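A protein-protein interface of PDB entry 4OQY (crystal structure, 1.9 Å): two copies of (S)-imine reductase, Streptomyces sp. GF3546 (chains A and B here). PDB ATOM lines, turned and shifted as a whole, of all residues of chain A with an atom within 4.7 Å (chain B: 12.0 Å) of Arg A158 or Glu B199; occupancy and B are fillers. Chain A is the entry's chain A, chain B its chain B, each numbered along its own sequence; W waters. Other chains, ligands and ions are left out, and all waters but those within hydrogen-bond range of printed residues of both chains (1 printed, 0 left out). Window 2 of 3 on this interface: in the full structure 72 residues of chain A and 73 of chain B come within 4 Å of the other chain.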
ATOM      1  N   TYR A 134     -17.920   0.245 -31.319  1.00  0.00           N
ATOM      2  CA  TYR A 134     -18.819  -0.761 -30.793  1.00  0.00           C
ATOM      3  C   TYR A 134     -20.066  -0.082 -30.261  1.00  0.00           C
ATOM      4  O   TYR A 134     -19.958   0.919 -29.564  1.00  0.00           O
ATOM      5  CB  TYR A 134     -18.172  -1.517 -29.624  1.00  0.00           C
ATOM      6  CG  TYR A 134     -16.854  -2.188 -29.930  1.00  0.00           C
ATOM      7  CD1 TYR A 134     -16.801  -3.282 -30.784  1.00  0.00           C
ATOM      8  CD2 TYR A 134     -15.668  -1.720 -29.387  1.00  0.00           C
ATOM      9  CE1 TYR A 134     -15.610  -3.902 -31.072  1.00  0.00           C
ATOM     10  CE2 TYR A 134     -14.458  -2.354 -29.665  1.00  0.00           C
ATOM     11  CZ  TYR A 134     -14.453  -3.441 -30.507  1.00  0.00           C
ATOM     12  OH  TYR A 134     -13.285  -4.095 -30.812  1.00  0.00           O
ATOM     13  N   TYR A 135     -21.241  -0.639 -30.556  1.00  0.00           N
ATOM     14  CA  TYR A 135     -22.498  -0.101 -30.038  1.00  0.00           C
ATOM     15  C   TYR A 135     -23.290  -1.202 -29.387  1.00  0.00           C
ATOM     16  O   TYR A 135     -23.291  -2.344 -29.860  1.00  0.00           O
ATOM     17  CB  TYR A 135     -23.354   0.571 -31.140  1.00  0.00           C
ATOM     18  CG  TYR A 135     -22.860   1.938 -31.503  1.00  0.00           C
ATOM     19  CD1 TYR A 135     -23.128   3.040 -30.699  1.00  0.00           C
ATOM     20  CD2 TYR A 135     -22.116   2.133 -32.651  1.00  0.00           C
ATOM     21  CE1 TYR A 135     -22.660   4.289 -31.031  1.00  0.00           C
ATOM     22  CE2 TYR A 135     -21.630   3.372 -32.974  1.00  0.00           C
ATOM     23  CZ  TYR A 135     -21.908   4.446 -32.166  1.00  0.00           C
ATOM     24  OH  TYR A 135     -21.416   5.666 -32.524  1.00  0.00           O
ATOM     25  N   ASP A 156     -20.768  -0.672 -35.147  1.00  0.00           N
ATOM     26  CA  ASP A 156     -20.763  -2.122 -35.064  1.00  0.00           C
ATOM     27  C   ASP A 156     -21.633  -2.517 -33.893  1.00  0.00           C
ATOM     28  O   ASP A 156     -21.188  -2.429 -32.757  1.00  0.00           O
ATOM     29  CB  ASP A 156     -19.327  -2.645 -34.938  1.00  0.00           C
ATOM     30  CG  ASP A 156     -19.241  -4.166 -34.853  1.00  0.00           C
ATOM     31  OD1 ASP A 156     -20.267  -4.864 -34.832  1.00  0.00           O
ATOM     32  OD2 ASP A 156     -18.120  -4.686 -34.770  1.00  0.00           O
ATOM     33  N   TYR A 157     -22.887  -2.895 -34.188  1.00  0.00           N
ATOM     34  CA  TYR A 157     -23.874  -3.243 -33.156  1.00  0.00           C
ATOM     35  C   TYR A 157     -23.565  -4.633 -32.616  1.00  0.00           C
ATOM     36  O   TYR A 157     -23.456  -5.589 -33.379  1.00  0.00           O
ATOM     37  CB  TYR A 157     -25.304  -3.194 -33.708  1.00  0.00           C
ATOM     38  CG  TYR A 157     -26.366  -3.539 -32.686  1.00  0.00           C
ATOM     39  CD1 TYR A 157     -26.785  -2.597 -31.755  1.00  0.00           C
ATOM     40  CD2 TYR A 157     -26.930  -4.808 -32.634  1.00  0.00           C
ATOM     41  CE1 TYR A 157     -27.747  -2.905 -30.812  1.00  0.00           C
ATOM     42  CE2 TYR A 157     -27.898  -5.126 -31.683  1.00  0.00           C
ATOM     43  CZ  TYR A 157     -28.301  -4.166 -30.773  1.00  0.00           C
ATOM     44  OH  TYR A 157     -29.258  -4.444 -29.816  1.00  0.00           O
ATOM     45  N   ARG A 158     -23.394  -4.726 -31.293  1.00  0.00           N
ATOM     46  CA  ARG A 158     -22.911  -5.951 -30.651  1.00  0.00           C
ATOM     47  C   ARG A 158     -23.967  -6.672 -29.813  1.00  0.00           C
ATOM     48  O   ARG A 158     -23.729  -7.796 -29.395  1.00  0.00           O
ATOM     49  CB  ARG A 158     -21.676  -5.661 -29.764  1.00  0.00           C
ATOM     50  CG  ARG A 158     -20.530  -4.946 -30.484  1.00  0.00           C
ATOM     51  CD  ARG A 158     -20.145  -5.556 -31.827  1.00  0.00           C
ATOM     52  NE  ARG A 158     -20.031  -6.998 -31.720  1.00  0.00           N
ATOM     53  CZ  ARG A 158     -20.460  -7.919 -32.572  1.00  0.00           C
ATOM     54  NH1 ARG A 158     -21.076  -7.638 -33.715  1.00  0.00           N
ATOM     55  NH2 ARG A 158     -20.249  -9.185 -32.253  1.00  0.00           N
ATOM     56  N   GLY A 159     -25.118  -6.042 -29.567  1.00  0.00           N
ATOM     57  CA  GLY A 159     -26.217  -6.686 -28.841  1.00  0.00           C
ATOM     58  C   GLY A 159     -27.026  -5.735 -27.977  1.00  0.00           C
ATOM     59  O   GLY A 159     -26.753  -4.550 -27.938  1.00  0.00           O
ATOM     60  N   LEU A 164     -22.310  -4.361 -23.149  1.00  0.00           N
ATOM     61  CA  LEU A 164     -21.547  -5.066 -24.180  1.00  0.00           C
ATOM     62  C   LEU A 164     -20.538  -4.197 -24.914  1.00  0.00           C
ATOM     63  O   LEU A 164     -19.399  -4.596 -25.075  1.00  0.00           O
ATOM     64  CB  LEU A 164     -22.488  -5.748 -25.198  1.00  0.00           C
ATOM     65  CG  LEU A 164     -23.163  -7.037 -24.719  1.00  0.00           C
ATOM     66  CD1 LEU A 164     -24.338  -7.438 -25.613  1.00  0.00           C
ATOM     67  CD2 LEU A 164     -22.168  -8.172 -24.637  1.00  0.00           C
ATOM     68  N   TYR A 168     -16.389  -4.738 -24.959  1.00  0.00           N
ATOM     69  CA  TYR A 168     -15.476  -4.877 -26.073  1.00  0.00           C
ATOM     70  C   TYR A 168     -14.371  -3.818 -25.983  1.00  0.00           C
ATOM     71  O   TYR A 168     -13.208  -4.111 -26.263  1.00  0.00           O
ATOM     72  CB  TYR A 168     -16.220  -4.749 -27.396  1.00  0.00           C
ATOM     73  CG  TYR A 168     -16.953  -5.978 -27.839  1.00  0.00           C
ATOM     74  CD1 TYR A 168     -18.174  -6.311 -27.296  1.00  0.00           C
ATOM     75  CD2 TYR A 168     -16.435  -6.793 -28.852  1.00  0.00           C
ATOM     76  CE1 TYR A 168     -18.860  -7.425 -27.729  1.00  0.00           C
ATOM     77  CE2 TYR A 168     -17.121  -7.906 -29.304  1.00  0.00           C
ATOM     78  CZ  TYR A 168     -18.330  -8.224 -28.731  1.00  0.00           C
ATOM     79  OH  TYR A 168     -19.026  -9.323 -29.177  1.00  0.00           O
ATOM     80  N   TYR B 183      -4.839 -11.941 -24.087  1.00  0.00           N
ATOM     81  CA  TYR B 183      -5.773 -12.446 -25.091  1.00  0.00           C
ATOM     82  C   TYR B 183      -6.754 -13.400 -24.427  1.00  0.00           C
ATOM     83  O   TYR B 183      -7.958 -13.192 -24.457  1.00  0.00           O
ATOM     84  CB  TYR B 183      -4.945 -13.133 -26.149  1.00  0.00           C
ATOM     85  CG  TYR B 183      -5.674 -13.827 -27.235  1.00  0.00           C
ATOM     86  CD1 TYR B 183      -6.130 -13.104 -28.306  1.00  0.00           C
ATOM     87  CD2 TYR B 183      -5.851 -15.213 -27.234  1.00  0.00           C
ATOM     88  CE1 TYR B 183      -6.765 -13.717 -29.361  1.00  0.00           C
ATOM     89  CE2 TYR B 183      -6.503 -15.843 -28.298  1.00  0.00           C
ATOM     90  CZ  TYR B 183      -6.958 -15.073 -29.344  1.00  0.00           C
ATOM     91  OH  TYR B 183      -7.618 -15.630 -30.430  1.00  0.00           O
ATOM     92  N   THR B 186      -9.222 -11.619 -22.054  1.00  0.00           N
ATOM     93  CA  THR B 186     -10.313 -11.013 -22.747  1.00  0.00           C
ATOM     94  C   THR B 186     -11.413 -12.032 -23.069  1.00  0.00           C
ATOM     95  O   THR B 186     -12.607 -11.715 -23.025  1.00  0.00           O
ATOM     96  CB  THR B 186      -9.739 -10.405 -24.053  1.00  0.00           C
ATOM     97  OG1 THR B 186      -9.136  -9.131 -23.763  1.00  0.00           O
ATOM     98  CG2 THR B 186     -10.756 -10.266 -25.072  1.00  0.00           C
ATOM     99  N   LEU B 187     -11.010 -13.252 -23.402  1.00  0.00           N
ATOM    100  CA  LEU B 187     -11.986 -14.275 -23.753  1.00  0.00           C
ATOM    101  C   LEU B 187     -12.742 -14.696 -22.485  1.00  0.00           C
ATOM    102  O   LEU B 187     -13.949 -14.908 -22.513  1.00  0.00           O
ATOM    103  CB  LEU B 187     -11.307 -15.458 -24.445  1.00  0.00           C
ATOM    104  CG  LEU B 187     -10.643 -15.185 -25.813  1.00  0.00           C
ATOM    105  CD1 LEU B 187      -9.990 -16.459 -26.338  1.00  0.00           C
ATOM    106  CD2 LEU B 187     -11.615 -14.632 -26.851  1.00  0.00           C
ATOM    107  N   ALA B 188     -12.029 -14.751 -21.362  1.00  0.00           N
ATOM    108  CA  ALA B 188     -12.651 -14.987 -20.071  1.00  0.00           C
ATOM    109  C   ALA B 188     -13.652 -13.883 -19.740  1.00  0.00           C
ATOM    110  O   ALA B 188     -14.791 -14.167 -19.391  1.00  0.00           O
ATOM    111  CB  ALA B 188     -11.589 -15.077 -18.976  1.00  0.00           C
ATOM    112  N   LEU B 189     -13.216 -12.630 -19.861  1.00  0.00           N
ATOM    113  CA  LEU B 189     -14.085 -11.475 -19.628  1.00  0.00           C
ATOM    114  C   LEU B 189     -15.321 -11.536 -20.532  1.00  0.00           C
ATOM    115  O   LEU B 189     -16.436 -11.302 -20.088  1.00  0.00           O
ATOM    116  CB  LEU B 189     -13.323 -10.154 -19.840  1.00  0.00           C
ATOM    117  CG  LEU B 189     -14.158  -8.867 -19.767  1.00  0.00           C
ATOM    118  CD1 LEU B 189     -14.601  -8.605 -18.333  1.00  0.00           C
ATOM    119  CD2 LEU B 189     -13.406  -7.669 -20.336  1.00  0.00           C
ATOM    120  N   GLY B 190     -15.118 -11.850 -21.803  1.00  0.00           N
ATOM    121  CA  GLY B 190     -16.247 -12.000 -22.722  1.00  0.00           C
ATOM    122  C   GLY B 190     -17.269 -13.010 -22.219  1.00  0.00           C
ATOM    123  O   GLY B 190     -18.475 -12.728 -22.152  1.00  0.00           O
ATOM    124  N   GLN B 191     -16.790 -14.193 -21.845  1.00  0.00           N
ATOM    125  CA  GLN B 191     -17.692 -15.264 -21.409  1.00  0.00           C
ATOM    126  C   GLN B 191     -18.455 -14.883 -20.168  1.00  0.00           C
ATOM    127  O   GLN B 191     -19.640 -15.161 -20.069  1.00  0.00           O
ATOM    128  CB  GLN B 191     -16.945 -16.570 -21.187  1.00  0.00           C
ATOM    129  CG  GLN B 191     -16.616 -17.246 -22.500  1.00  0.00           C
ATOM    130  CD  GLN B 191     -15.719 -18.458 -22.353  1.00  0.00           C
ATOM    131  OE1 GLN B 191     -15.338 -18.845 -21.255  1.00  0.00           O
ATOM    132  NE2 GLN B 191     -15.377 -19.067 -23.487  1.00  0.00           N
ATOM    133  N   ALA B 192     -17.793 -14.202 -19.249  1.00  0.00           N
ATOM    134  CA  ALA B 192     -18.443 -13.740 -18.036  1.00  0.00           C
ATOM    135  C   ALA B 192     -19.519 -12.691 -18.317  1.00  0.00           C
ATOM    136  O   ALA B 192     -20.318 -12.381 -17.435  1.00  0.00           O
ATOM    137  CB  ALA B 192     -17.409 -13.174 -17.069  1.00  0.00           C
ATOM    138  N   ASN B 193     -19.520 -12.122 -19.530  1.00  0.00           N
ATOM    139  CA  ASN B 193     -20.505 -11.111 -19.955  1.00  0.00           C
ATOM    140  C   ASN B 193     -21.447 -11.662 -21.019  1.00  0.00           C
ATOM    141  O   ASN B 193     -22.130 -10.905 -21.703  1.00  0.00           O
ATOM    142  CB  ASN B 193     -19.800  -9.858 -20.497  1.00  0.00           C
ATOM    143  CG  ASN B 193     -19.328  -8.924 -19.397  1.00  0.00           C
ATOM    144  OD1 ASN B 193     -20.085  -8.078 -18.919  1.00  0.00           O
ATOM    145  ND2 ASN B 193     -18.076  -9.077 -18.982  1.00  0.00           N
ATOM    146  N   GLY B 194     -21.476 -12.983 -21.165  1.00  0.00           N
ATOM    147  CA  GLY B 194     -22.374 -13.643 -22.107  1.00  0.00           C
ATOM    148  C   GLY B 194     -21.968 -13.627 -23.571  1.00  0.00           C
ATOM    149  O   GLY B 194     -22.796 -13.886 -24.446  1.00  0.00           O
ATOM    150  N   VAL B 195     -20.705 -13.324 -23.856  1.00  0.00           N
ATOM    151  CA  VAL B 195     -20.197 -13.370 -25.227  1.00  0.00           C
ATOM    152  C   VAL B 195     -19.297 -14.587 -25.369  1.00  0.00           C
ATOM    153  O   VAL B 195     -18.301 -14.714 -24.654  1.00  0.00           O
ATOM    154  CB  VAL B 195     -19.432 -12.088 -25.599  1.00  0.00           C
ATOM    155  CG1 VAL B 195     -19.025 -12.101 -27.067  1.00  0.00           C
ATOM    156  CG2 VAL B 195     -20.286 -10.868 -25.290  1.00  0.00           C
ATOM    157  N   SER B 196     -19.655 -15.460 -26.311  1.00  0.00           N
ATOM    158  CA  SER B 196     -18.941 -16.701 -26.510  1.00  0.00           C
ATOM    159  C   SER B 196     -17.567 -16.420 -27.057  1.00  0.00           C
ATOM    160  O   SER B 196     -17.344 -15.426 -27.747  1.00  0.00           O
ATOM    161  CB  SER B 196     -19.674 -17.601 -27.495  1.00  0.00           C
ATOM    162  OG  SER B 196     -19.419 -17.171 -28.817  1.00  0.00           O
ATOM    163  N   ALA B 197     -16.649 -17.323 -26.746  1.00  0.00           N
ATOM    164  CA  ALA B 197     -15.262 -17.176 -27.146  1.00  0.00           C
ATOM    165  C   ALA B 197     -15.176 -17.127 -28.660  1.00  0.00           C
ATOM    166  O   ALA B 197     -14.371 -16.387 -29.206  1.00  0.00           O
ATOM    167  CB  ALA B 197     -14.405 -18.304 -26.577  1.00  0.00           C
ATOM    168  N   LYS B 198     -16.040 -17.866 -29.344  1.00  0.00           N
ATOM    169  CA  LYS B 198     -15.980 -17.884 -30.796  1.00  0.00           C
ATOM    170  C   LYS B 198     -16.507 -16.593 -31.419  1.00  0.00           C
ATOM    171  O   LYS B 198     -15.987 -16.135 -32.436  1.00  0.00           O
ATOM    172  CB  LYS B 198     -16.661 -19.140 -31.359  1.00  0.00           C
ATOM    173  CG  LYS B 198     -18.146 -19.064 -31.673  1.00  0.00           C
ATOM    174  CD  LYS B 198     -18.699 -20.470 -31.910  1.00  0.00           C
ATOM    175  CE  LYS B 198     -20.168 -20.606 -31.530  1.00  0.00           C
ATOM    176  NZ  LYS B 198     -21.086 -20.263 -32.652  1.00  0.00           N
ATOM    177  N   GLU B 199     -17.505 -15.984 -30.798  1.00  0.00           N
ATOM    178  CA  GLU B 199     -17.972 -14.683 -31.256  1.00  0.00           C
ATOM    179  C   GLU B 199     -16.941 -13.573 -30.966  1.00  0.00           C
ATOM    180  O   GLU B 199     -16.738 -12.667 -31.776  1.00  0.00           O
ATOM    181  CB  GLU B 199     -19.317 -14.352 -30.614  1.00  0.00           C
ATOM    182  CG  GLU B 199     -19.846 -12.963 -30.943  1.00  0.00           C
ATOM    183  CD  GLU B 199     -21.285 -12.752 -30.498  1.00  0.00           C
ATOM    184  OE1 GLU B 199     -22.022 -13.750 -30.311  1.00  0.00           O
ATOM    185  OE2 GLU B 199     -21.695 -11.579 -30.368  1.00  0.00           O
ATOM    186  N   LEU B 200     -16.283 -13.637 -29.816  1.00  0.00           N
ATOM    187  CA  LEU B 200     -15.274 -12.619 -29.473  1.00  0.00           C
ATOM    188  C   LEU B 200     -13.916 -12.854 -30.147  1.00  0.00           C
ATOM    189  O   LEU B 200     -13.147 -11.912 -30.352  1.00  0.00           O
ATOM    190  CB  LEU B 200     -15.083 -12.566 -27.955  1.00  0.00           C
ATOM    191  CG  LEU B 200     -14.269 -11.414 -27.375  1.00  0.00           C
ATOM    192  CD1 LEU B 200     -14.844 -10.048 -27.722  1.00  0.00           C
ATOM    193  CD2 LEU B 200     -14.225 -11.589 -25.868  1.00  0.00           C
ATOM    194  N   LEU B 201     -13.633 -14.112 -30.495  1.00  0.00           N
ATOM    195  CA  LEU B 201     -12.320 -14.508 -31.033  1.00  0.00           C
ATOM    196  C   LEU B 201     -11.753 -13.592 -32.146  1.00  0.00           C
ATOM    197  O   LEU B 201     -10.633 -13.116 -32.016  1.00  0.00           O
ATOM    198  CB  LEU B 201     -12.334 -15.975 -31.508  1.00  0.00           C
ATOM    199  CG  LEU B 201     -10.965 -16.661 -31.486  1.00  0.00           C
ATOM    200  CD1 LEU B 201     -10.497 -16.911 -30.049  1.00  0.00           C
ATOM    201  CD2 LEU B 201     -10.983 -17.965 -32.270  1.00  0.00           C
ATOM    202  N   PRO B 202     -12.522 -13.337 -33.229  1.00  0.00           N
ATOM    203  CA  PRO B 202     -12.002 -12.439 -34.263  1.00  0.00           C
ATOM    204  C   PRO B 202     -11.664 -11.041 -33.739  1.00  0.00           C
ATOM    205  O   PRO B 202     -10.658 -10.468 -34.136  1.00  0.00           O
ATOM    206  CB  PRO B 202     -13.135 -12.386 -35.302  1.00  0.00           C
ATOM    207  CG  PRO B 202     -14.351 -12.863 -34.587  1.00  0.00           C
ATOM    208  CD  PRO B 202     -13.856 -13.854 -33.580  1.00  0.00           C
ATOM    209  N   TYR B 203     -12.472 -10.510 -32.827  1.00  0.00           N
ATOM    210  CA  TYR B 203     -12.164  -9.206 -32.219  1.00  0.00           C
ATOM    211  C   TYR B 203     -10.879  -9.225 -31.393  1.00  0.00           C
ATOM    212  O   TYR B 203     -10.002  -8.350 -31.548  1.00  0.00           O
ATOM    213  CB  TYR B 203     -13.332  -8.732 -31.354  1.00  0.00           C
ATOM    214  CG  TYR B 203     -14.533  -8.352 -32.176  1.00  0.00           C
ATOM    215  CD1 TYR B 203     -14.613  -7.100 -32.770  1.00  0.00           C
ATOM    216  CD2 TYR B 203     -15.573  -9.247 -32.385  1.00  0.00           C
ATOM    217  CE1 TYR B 203     -15.703  -6.739 -33.537  1.00  0.00           C
ATOM    218  CE2 TYR B 203     -16.673  -8.899 -33.160  1.00  0.00           C
ATOM    219  CZ  TYR B 203     -16.726  -7.641 -33.736  1.00  0.00           C
ATOM    220  OH  TYR B 203     -17.807  -7.262 -34.483  1.00  0.00           O
ATOM    221  N   ALA B 204     -10.769 -10.217 -30.510  1.00  0.00           N
ATOM    222  CA  ALA B 204      -9.571 -10.351 -29.655  1.00  0.00           C
ATOM    223  C   ALA B 204      -8.319 -10.487 -30.545  1.00  0.00           C
ATOM    224  O   ALA B 204      -7.254  -9.945 -30.230  1.00  0.00           O
ATOM    225  CB  ALA B 204      -9.709 -11.541 -28.710  1.00  0.00           C
ATOM    226  N   THR B 205      -8.485 -11.163 -31.684  1.00  0.00           N
ATOM    227  CA  THR B 205      -7.392 -11.380 -32.607  1.00  0.00           C
ATOM    228  C   THR B 205      -6.987 -10.052 -33.188  1.00  0.00           C
ATOM    229  O   THR B 205      -5.812  -9.715 -33.158  1.00  0.00           O
ATOM    230  CB  THR B 205      -7.781 -12.370 -33.730  1.00  0.00           C
ATOM    231  OG1 THR B 205      -8.058 -13.643 -33.146  1.00  0.00           O
ATOM    232  CG2 THR B 205      -6.658 -12.530 -34.737  1.00  0.00           C
ATOM    233  N   MET B 206      -7.949  -9.297 -33.707  1.00  0.00           N
ATOM    234  CA  MET B 206      -7.653  -7.975 -34.246  1.00  0.00           C
ATOM    235  C   MET B 206      -7.072  -7.045 -33.181  1.00  0.00           C
ATOM    236  O   MET B 206      -6.264  -6.167 -33.497  1.00  0.00           O
ATOM    237  CB  MET B 206      -8.894  -7.334 -34.890  1.00  0.00           C
ATOM    238  CG  MET B 206      -8.909  -5.807 -34.983  1.00  0.00           C
ATOM    239  SD  MET B 206      -9.723  -4.880 -33.632  1.00  0.00           S
ATOM    240  CE  MET B 206      -8.543  -3.615 -33.126  1.00  0.00           C
ATOM    241  N   MET B 207      -7.516  -7.202 -31.939  1.00  0.00           N
ATOM    242  CA  MET B 207      -7.039  -6.320 -30.882  1.00  0.00           C
ATOM    243  C   MET B 207      -5.545  -6.472 -30.669  1.00  0.00           C
ATOM    244  O   MET B 207      -4.905  -5.521 -30.221  1.00  0.00           O
ATOM    245  CB  MET B 207      -7.786  -6.572 -29.585  1.00  0.00           C
ATOM    246  CG  MET B 207      -9.209  -6.042 -29.581  1.00  0.00           C
ATOM    247  SD  MET B 207     -10.181  -6.747 -28.249  1.00  0.00           S
ATOM    248  CE  MET B 207     -11.842  -6.205 -28.609  1.00  0.00           C
HETATM  249  O   HOH W   1     -21.668  -9.417 -28.535  1.00  0.00           O
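Of the 23 printed residues of chain B, 5 touch a printed residue of chain A.
Hydrophobic or aromatic side chains of chain B that line the printed part of chain A: Val B195, Leu B200, Tyr B203 and Met B207.
Of the 8 printed residues of chain A, 5 touch a printed residue of chain B.
Along chain A the printed residues that touch a printed residue of chain B span positions 134 to 168.
N of Tyr A135 lies within hydrogen-bond range of O of Asp A156 (2.8 Å).
O of Tyr A135 lies within hydrogen-bond range of N of Arg A158, 2.8 Å away.
The side-chain carboxylate (OD1) of Asp A156 is in salt-bridge range of the guanidinium group (NH1) of Arg A158.
The guanidinium group (NH2) of Arg A158 sits at hydrogen-bond distance from the side-chain hydroxyl (OH) of Tyr A168 (3.3 Å).
The backbone carbonyl oxygen (O) of Gly B190 lies within hydrogen-bond range of the backbone NH (N) of Val B195 (2.9 Å).
The backbone NH (N) of Glu B199 lies within hydrogen-bond range of the side-chain hydroxyl (OG) of Ser B196, at 3.0 Å.
Water W1 lies within hydrogen-bond range of OH of Tyr A168 (2.7 Å), O of Arg A158 (2.8 Å) and OE2 of Glu B199 (2.8 Å).
OD2 of Asp A156 sits at hydrogen-bond distance from OH of Tyr B203, 2.6 Å away.
The side-chain carboxylate of Glu B199 lies within salt-bridge range of the guanidinium group of Arg A158.
NH1 of Arg A158 sits close to OH of Tyr B203 (3.4 Å).
Tyr A134 touches just these residues of chain B: Tyr B203 and Met B207.
Asp A156 touches just one residue of chain B: Tyr B203.
No residue of chain B comes within 4 Å of Tyr A157.
Arg A158 touches two residues of chain B.
No residue of chain B comes within 4 Å of Gly A159.
Of the printed residues of chain B, Tyr A168 touches Val B195, Glu B199, Leu B200, Tyr B203 and Met B207.
Gly B194 touches none of the printed residues of chain A.
Printed residues of chain A within 4 Å of Val B195: Leu A164 and Tyr A168.
Glu B199 touches two residues of chain A.
Of the printed residues of chain A, Tyr B203 touches Tyr A134 (3.8 Å), Asp A156 (2.6 Å), Arg A158 (3.3 Å) and Tyr A168 (3.7 Å).
Printed residues of chain A within 4 Å of Met B207: Tyr A134 and Tyr A168.
The nearest residue of chain B that does not touch Arg A158 is Val B195 (6.1 Å).
The nearest printed residue of chain A that does not touch Glu B199 is Gly A159 (6.6 Å).
The nearest printed residue of chain A that does not touch Val B195 is Arg A158 (6.1 Å).
CD1 of Tyr B203 touches CE1 of Tyr A134, at 3.8 Å.
CE of Met B207 touches OH of Tyr A134, at 3.4 Å.
Val B195 touches Leu A164 (CG2 to CD2, 3.4 Å).
Tyr A168 touches Val B195.
OE2 of Glu B199 touches OH of Tyr A168, at 3.7 Å.
Tyr A168 touches Leu B200 (CE2 to CD1, 3.5 Å).
CE2 of Tyr A168 touches CD2 of Tyr B203, 3.7 Å away.
Tyr A168 touches Met B207.
No position is printed for both chains.
Of the 11 pairs that touch across the chains among the printed residues, none has its exchanged pair printed and touching as well.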
